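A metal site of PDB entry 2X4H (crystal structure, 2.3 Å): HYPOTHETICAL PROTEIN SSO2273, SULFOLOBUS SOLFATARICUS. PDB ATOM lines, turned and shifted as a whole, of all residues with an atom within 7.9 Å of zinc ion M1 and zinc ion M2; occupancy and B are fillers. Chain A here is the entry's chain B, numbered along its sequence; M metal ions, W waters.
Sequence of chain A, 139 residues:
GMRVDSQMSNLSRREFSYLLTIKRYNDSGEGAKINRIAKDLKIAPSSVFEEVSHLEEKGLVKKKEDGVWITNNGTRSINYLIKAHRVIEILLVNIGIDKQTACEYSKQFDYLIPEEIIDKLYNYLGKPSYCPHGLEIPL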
ATOM      1  N   ARG A  13       6.196 -11.896  14.931  1.00  0.00           N
ATOM      2  CA  ARG A  13       6.216 -10.542  15.440  1.00  0.00           C
ATOM      3  C   ARG A  13       5.647 -10.445  16.839  1.00  0.00           C
ATOM      4  O   ARG A  13       6.040  -9.578  17.611  1.00  0.00           O
ATOM      5  CB  ARG A  13       5.556  -9.561  14.471  1.00  0.00           C
ATOM      6  CG  ARG A  13       6.614  -8.859  13.678  1.00  0.00           C
ATOM      7  CD  ARG A  13       6.082  -7.889  12.641  1.00  0.00           C
ATOM      8  NE  ARG A  13       7.191  -7.168  12.044  1.00  0.00           N
ATOM      9  CZ  ARG A  13       7.871  -6.177  12.653  1.00  0.00           C
ATOM     10  NH1 ARG A  13       7.530  -5.766  13.844  1.00  0.00           N
ATOM     11  NH2 ARG A  13       8.896  -5.587  12.022  1.00  0.00           N
ATOM     12  N   ILE A  82      15.023  -6.810  13.080  1.00  0.00           N
ATOM     13  CA  ILE A  82      15.147  -5.387  12.886  1.00  0.00           C
ATOM     14  C   ILE A  82      15.848  -5.140  11.532  1.00  0.00           C
ATOM     15  O   ILE A  82      15.398  -4.328  10.737  1.00  0.00           O
ATOM     16  CB  ILE A  82      15.949  -4.735  14.024  1.00  0.00           C
ATOM     17  CG1 ILE A  82      15.103  -4.633  15.300  1.00  0.00           C
ATOM     18  CG2 ILE A  82      16.501  -3.312  13.560  1.00  0.00           C
ATOM     19  CD1 ILE A  82      15.948  -4.219  16.613  1.00  0.00           C
ATOM     20  N   HIS A  85      13.465  -5.982   8.700  1.00  0.00           N
ATOM     21  CA  HIS A  85      12.479  -4.925   8.566  1.00  0.00           C
ATOM     22  C   HIS A  85      13.060  -3.732   7.794  1.00  0.00           C
ATOM     23  O   HIS A  85      12.469  -3.251   6.833  1.00  0.00           O
ATOM     24  CB  HIS A  85      12.008  -4.455   9.927  1.00  0.00           C
ATOM     25  CG  HIS A  85      11.062  -3.317   9.860  1.00  0.00           C
ATOM     26  ND1 HIS A  85       9.797  -3.423   9.332  1.00  0.00           N
ATOM     27  CD2 HIS A  85      11.218  -2.020  10.206  1.00  0.00           C
ATOM     28  CE1 HIS A  85       9.203  -2.251   9.393  1.00  0.00           C
ATOM     29  NE2 HIS A  85      10.050  -1.370   9.894  1.00  0.00           N
ATOM     30  N   ARG A  86      14.242  -3.322   8.215  1.00  0.00           N
ATOM     31  CA  ARG A  86      14.902  -2.139   7.671  1.00  0.00           C
ATOM     32  C   ARG A  86      15.498  -2.338   6.285  1.00  0.00           C
ATOM     33  O   ARG A  86      15.359  -1.474   5.437  1.00  0.00           O
ATOM     34  CB  ARG A  86      15.922  -1.613   8.695  1.00  0.00           C
ATOM     35  CG  ARG A  86      15.225  -1.166   9.947  1.00  0.00           C
ATOM     36  CD  ARG A  86      16.128  -0.566  11.002  1.00  0.00           C
ATOM     37  NE  ARG A  86      15.272  -0.162  12.114  1.00  0.00           N
ATOM     38  CZ  ARG A  86      15.645   0.121  13.345  1.00  0.00           C
ATOM     39  NH1 ARG A  86      16.918   0.099  13.750  1.00  0.00           N
ATOM     40  NH2 ARG A  86      14.695   0.439  14.191  1.00  0.00           N
ATOM     41  N   VAL A  87      16.090  -3.486   6.024  1.00  0.00           N
ATOM     42  CA  VAL A  87      16.554  -3.780   4.681  1.00  0.00           C
ATOM     43  C   VAL A  87      15.366  -3.835   3.673  1.00  0.00           C
ATOM     44  O   VAL A  87      15.458  -3.320   2.562  1.00  0.00           O
ATOM     45  CB  VAL A  87      17.325  -5.113   4.653  1.00  0.00           C
ATOM     46  CG1 VAL A  87      17.570  -5.581   3.197  1.00  0.00           C
ATOM     47  CG2 VAL A  87      18.651  -4.965   5.425  1.00  0.00           C
ATOM     48  N   GLU A  89      12.562  -2.278   3.896  1.00  0.00           N
ATOM     49  CA  GLU A  89      12.070  -0.910   3.753  1.00  0.00           C
ATOM     50  C   GLU A  89      12.835  -0.208   2.661  1.00  0.00           C
ATOM     51  O   GLU A  89      12.248   0.517   1.881  1.00  0.00           O
ATOM     52  CB  GLU A  89      12.257  -0.114   5.037  1.00  0.00           C
ATOM     53  CG  GLU A  89      11.133  -0.238   5.946  1.00  0.00           C
ATOM     54  CD  GLU A  89      11.229   0.654   7.174  1.00  0.00           C
ATOM     55  OE1 GLU A  89      10.214   0.663   7.892  1.00  0.00           O
ATOM     56  OE2 GLU A  89      12.301   1.261   7.478  1.00  0.00           O
ATOM     57  N   ILE A  90      14.147  -0.426   2.639  1.00  0.00           N
ATOM     58  CA  ILE A  90      14.993   0.218   1.674  1.00  0.00           C
ATOM     59  C   ILE A  90      14.632  -0.227   0.266  1.00  0.00           C
ATOM     60  O   ILE A  90      14.501   0.615  -0.620  1.00  0.00           O
ATOM     61  CB  ILE A  90      16.482  -0.023   1.986  1.00  0.00           C
ATOM     62  CG1 ILE A  90      16.866   0.741   3.251  1.00  0.00           C
ATOM     63  CG2 ILE A  90      17.366   0.467   0.820  1.00  0.00           C
ATOM     64  CD1 ILE A  90      18.302   0.619   3.589  1.00  0.00           C
ATOM     65  N   LYS A  99       7.632   5.921   2.258  1.00  0.00           N
ATOM     66  CA  LYS A  99       8.336   5.272   3.387  1.00  0.00           C
ATOM     67  C   LYS A  99       7.432   4.858   4.547  1.00  0.00           C
ATOM     68  O   LYS A  99       7.716   3.882   5.239  1.00  0.00           O
ATOM     69  CB  LYS A  99       9.473   6.145   3.949  1.00  0.00           C
ATOM     70  CG  LYS A  99       9.042   7.472   4.555  1.00  0.00           C
ATOM     71  CD  LYS A  99      10.205   8.138   5.318  1.00  0.00           C
ATOM     72  CE  LYS A  99       9.803   9.480   5.894  1.00  0.00           C
ATOM     73  NZ  LYS A  99      10.995  10.320   6.209  1.00  0.00           N
ATOM     74  N   GLN A 100       6.349   5.592   4.768  1.00  0.00           N
ATOM     75  CA  GLN A 100       5.369   5.177   5.770  1.00  0.00           C
ATOM     76  C   GLN A 100       4.640   3.881   5.319  1.00  0.00           C
ATOM     77  O   GLN A 100       4.489   2.958   6.112  1.00  0.00           O
ATOM     78  CB  GLN A 100       4.416   6.327   6.084  1.00  0.00           C
ATOM     79  CG  GLN A 100       3.367   6.028   7.113  1.00  0.00           C
ATOM     80  CD  GLN A 100       3.948   5.473   8.389  1.00  0.00           C
ATOM     81  OE1 GLN A 100       3.574   4.378   8.842  1.00  0.00           O
ATOM     82  NE2 GLN A 100       4.879   6.204   8.978  1.00  0.00           N
ATOM     83  N   ALA A 102       5.847   1.748   3.148  1.00  0.00           N
ATOM     84  CA  ALA A 102       6.910   0.771   3.127  1.00  0.00           C
ATOM     85  C   ALA A 102       7.068   0.128   4.495  1.00  0.00           C
ATOM     86  O   ALA A 102       7.232  -1.083   4.577  1.00  0.00           O
ATOM     87  CB  ALA A 102       8.229   1.447   2.713  1.00  0.00           C
ATOM     88  N   CYS A 103       7.040   0.950   5.555  1.00  0.00           N
ATOM     89  CA  CYS A 103       7.160   0.454   6.924  1.00  0.00           C
ATOM     90  C   CYS A 103       6.014  -0.503   7.200  1.00  0.00           C
ATOM     91  O   CYS A 103       6.246  -1.614   7.629  1.00  0.00           O
ATOM     92  CB  CYS A 103       7.173   1.613   7.953  1.00  0.00           C
ATOM     93  SG  CYS A 103       7.746   1.126   9.626  1.00  0.00           S
ATOM     94  N   GLU A 104       4.785  -0.077   6.907  1.00  0.00           N
ATOM     95  CA  GLU A 104       3.598  -0.887   7.212  1.00  0.00           C
ATOM     96  C   GLU A 104       3.625  -2.215   6.451  1.00  0.00           C
ATOM     97  O   GLU A 104       3.355  -3.274   7.021  1.00  0.00           O
ATOM     98  CB  GLU A 104       2.326  -0.102   6.864  1.00  0.00           C
ATOM     99  CG  GLU A 104       2.027   1.052   7.803  1.00  0.00           C
ATOM    100  CD  GLU A 104       1.038   2.120   7.244  1.00  0.00           C
ATOM    101  OE1 GLU A 104       0.613   2.031   6.057  1.00  0.00           O
ATOM    102  OE2 GLU A 104       0.687   3.054   8.002  1.00  0.00           O
ATOM    103  N   SER A 106       6.332  -3.713   5.172  1.00  0.00           N
ATOM    104  CA  SER A 106       7.434  -4.530   5.644  1.00  0.00           C
ATOM    105  C   SER A 106       7.006  -5.376   6.864  1.00  0.00           C
ATOM    106  O   SER A 106       7.292  -6.540   6.909  1.00  0.00           O
ATOM    107  CB  SER A 106       8.652  -3.658   5.992  1.00  0.00           C
ATOM    108  OG  SER A 106       9.821  -4.431   6.117  1.00  0.00           O
ATOM    109  N   LYS A 107       6.287  -4.781   7.803  1.00  0.00           N
ATOM    110  CA  LYS A 107       5.841  -5.514   9.011  1.00  0.00           C
ATOM    111  C   LYS A 107       4.968  -6.735   8.693  1.00  0.00           C
ATOM    112  O   LYS A 107       4.868  -7.612   9.519  1.00  0.00           O
ATOM    113  CB  LYS A 107       5.073  -4.601   9.974  1.00  0.00           C
ATOM    114  CG  LYS A 107       5.920  -3.530  10.657  1.00  0.00           C
ATOM    115  CD  LYS A 107       5.096  -2.673  11.636  1.00  0.00           C
ATOM    116  CE  LYS A 107       5.858  -1.439  12.131  1.00  0.00           C
ATOM    117  NZ  LYS A 107       6.646  -1.672  13.376  1.00  0.00           N
ATOM    118  N   ASP A 110       8.178  -9.285   6.852  1.00  0.00           N
ATOM    119  CA  ASP A 110       9.626  -9.288   7.136  1.00  0.00           C
ATOM    120  C   ASP A 110      10.062 -10.473   7.971  1.00  0.00           C
ATOM    121  O   ASP A 110      11.063 -11.106   7.672  1.00  0.00           O
ATOM    122  CB  ASP A 110      10.122  -7.984   7.783  1.00  0.00           C
ATOM    123  CG  ASP A 110       9.275  -7.547   8.953  1.00  0.00           C
ATOM    124  OD1 ASP A 110       8.444  -8.335   9.457  1.00  0.00           O
ATOM    125  OD2 ASP A 110       9.409  -6.379   9.351  1.00  0.00           O
ATOM    126  N   TYR A 130      21.483   2.777   7.435  1.00  0.00           N
ATOM    127  CA  TYR A 130      20.261   3.284   8.079  1.00  0.00           C
ATOM    128  C   TYR A 130      19.096   3.091   7.187  1.00  0.00           C
ATOM    129  O   TYR A 130      19.252   3.141   5.990  1.00  0.00           O
ATOM    130  CB  TYR A 130      20.382   4.777   8.400  1.00  0.00           C
ATOM    131  CG  TYR A 130      21.431   5.098   9.418  1.00  0.00           C
ATOM    132  CD1 TYR A 130      21.104   5.233  10.757  1.00  0.00           C
ATOM    133  CD2 TYR A 130      22.757   5.315   9.040  1.00  0.00           C
ATOM    134  CE1 TYR A 130      22.107   5.572  11.722  1.00  0.00           C
ATOM    135  CE2 TYR A 130      23.753   5.645   9.974  1.00  0.00           C
ATOM    136  CZ  TYR A 130      23.417   5.770  11.311  1.00  0.00           C
ATOM    137  OH  TYR A 130      24.391   6.056  12.215  1.00  0.00           O
ATOM    138  N   CYS A 131      17.922   2.857   7.780  1.00  0.00           N
ATOM    139  CA  CYS A 131      16.683   2.744   7.016  1.00  0.00           C
ATOM    140  C   CYS A 131      16.164   4.148   6.688  1.00  0.00           C
ATOM    141  O   CYS A 131      16.706   5.129   7.207  1.00  0.00           O
ATOM    142  CB  CYS A 131      15.658   1.943   7.830  1.00  0.00           C
ATOM    143  SG  CYS A 131      14.829   2.883   9.142  1.00  0.00           S
ATOM    144  N   PRO A 132      15.136   4.276   5.834  1.00  0.00           N
ATOM    145  CA  PRO A 132      14.657   5.619   5.461  1.00  0.00           C
ATOM    146  C   PRO A 132      14.164   6.493   6.619  1.00  0.00           C
ATOM    147  O   PRO A 132      14.065   7.683   6.469  1.00  0.00           O
ATOM    148  CB  PRO A 132      13.524   5.353   4.456  1.00  0.00           C
ATOM    149  CG  PRO A 132      13.675   3.945   4.016  1.00  0.00           C
ATOM    150  CD  PRO A 132      14.302   3.224   5.212  1.00  0.00           C
ATOM    151  N   HIS A 133      13.857   5.899   7.774  1.00  0.00           N
ATOM    152  CA  HIS A 133      13.504   6.663   8.969  1.00  0.00           C
ATOM    153  C   HIS A 133      14.744   7.045   9.779  1.00  0.00           C
ATOM    154  O   HIS A 133      14.638   7.481  10.923  1.00  0.00           O
ATOM    155  CB  HIS A 133      12.516   5.859   9.850  1.00  0.00           C
ATOM    156  CG  HIS A 133      11.397   5.253   9.065  1.00  0.00           C
ATOM    157  ND1 HIS A 133      11.276   3.891   8.845  1.00  0.00           N
ATOM    158  CD2 HIS A 133      10.361   5.840   8.420  1.00  0.00           C
ATOM    159  CE1 HIS A 133      10.224   3.679   8.077  1.00  0.00           C
ATOM    160  NE2 HIS A 133       9.652   4.838   7.798  1.00  0.00           N
ATOM    161  N   GLY A 134      15.941   6.856   9.221  1.00  0.00           N
ATOM    162  CA  GLY A 134      17.173   7.220   9.910  1.00  0.00           C
ATOM    163  C   GLY A 134      17.518   6.327  11.072  1.00  0.00           C
ATOM    164  O   GLY A 134      18.213   6.748  11.983  1.00  0.00           O
ATOM    165  N   LEU A 135      17.054   5.086  11.080  1.00  0.00           N
ATOM    166  CA  LEU A 135      17.313   4.180  12.194  1.00  0.00           C
ATOM    167  C   LEU A 135      18.336   3.113  11.771  1.00  0.00           C
ATOM    168  O   LEU A 135      18.311   2.640  10.654  1.00  0.00           O
ATOM    169  CB  LEU A 135      16.003   3.547  12.676  1.00  0.00           C
ATOM    170  CG  LEU A 135      14.935   4.515  13.236  1.00  0.00           C
ATOM    171  CD1 LEU A 135      13.557   3.788  13.396  1.00  0.00           C
ATOM    172  CD2 LEU A 135      15.372   5.160  14.544  1.00  0.00           C
ATOM    173  N   GLU A 136      19.211   2.725  12.694  1.00  0.00           N
ATOM    174  CA  GLU A 136      20.433   1.964  12.362  1.00  0.00           C
ATOM    175  C   GLU A 136      20.106   0.542  11.953  1.00  0.00           C
ATOM    176  O   GLU A 136      19.283  -0.087  12.593  1.00  0.00           O
ATOM    177  CB  GLU A 136      21.427   1.975  13.531  1.00  0.00           C
ATOM    178  CG  GLU A 136      22.900   2.189  13.120  1.00  0.00           C
ATOM    179  CD  GLU A 136      23.839   2.661  14.263  1.00  0.00           C
ATOM    180  OE1 GLU A 136      23.376   3.128  15.333  1.00  0.00           O
ATOM    181  OE2 GLU A 136      25.069   2.573  14.066  1.00  0.00           O
ATOM    182  N   ILE A 137      20.734   0.061  10.882  1.00  0.00           N
ATOM    183  CA  ILE A 137      20.590  -1.314  10.454  1.00  0.00           C
ATOM    184  C   ILE A 137      21.753  -2.156  10.998  1.00  0.00           C
ATOM    185  O   ILE A 137      22.875  -1.861  10.704  1.00  0.00           O
ATOM    186  CB  ILE A 137      20.607  -1.429   8.942  1.00  0.00           C
ATOM    187  CG1 ILE A 137      19.479  -0.591   8.318  1.00  0.00           C
ATOM    188  CG2 ILE A 137      20.538  -2.874   8.544  1.00  0.00           C
ATOM    189  CD1 ILE A 137      19.339  -0.714   6.771  1.00  0.00           C
HETATM  190 ZN    ZN M   1       9.881   0.620   9.785  1.00  0.00          ZN
HETATM  191 ZN    ZN M   2      12.483   2.450   8.946  1.00  0.00          ZN
HETATM  192  O   HOH W   1      11.254   2.244  10.509  1.00  0.00           O
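A ring nitrogen (NE2) of His 133 is in hydrogen-bond range of the backbone carbonyl oxygen (O) of Lys 99, at 3.3 Å. The backbone carbonyl oxygen (O) of His 85 lies within hydrogen-bond range of the side-chain hydroxyl (OG) of Ser 106. A ring nitrogen (ND1) of His 85 is in hydrogen-bond range of the side-chain carboxylate of Asp 110 (3.0 Å). SG of Cys 131 lies close to N of Leu 135.
Within 4 Å of zinc ion M1: His 85, Glu 89, Cys 103 and His 133. The nearest printed residue that does not touch zinc ion M1 is Lys 107 (5.1 Å).
Of the 23 residues printed, 3 come within 4 Å of zinc ion M2. The nearest printed residue that does not touch zinc ion M2 is Pro 132 (4.2 Å).
Zinc ion M1 is bound by the side-chain carboxylate (OE1) of Glu 89, a ring nitrogen (NE2) of His 85, the side-chain sulfur (SG) of Cys 103 and water W1.
ND1 of His 133 is bound to zinc ion M2, 1.9 Å away. Zinc ion M2 is bound by OE2 of Glu 89, 1.9 Å away. Zinc ion M2 is bound by water W1 (2.0 Å). The side-chain sulfur (SG) of Cys 131 binds zinc ion M2 (2.4 Å).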
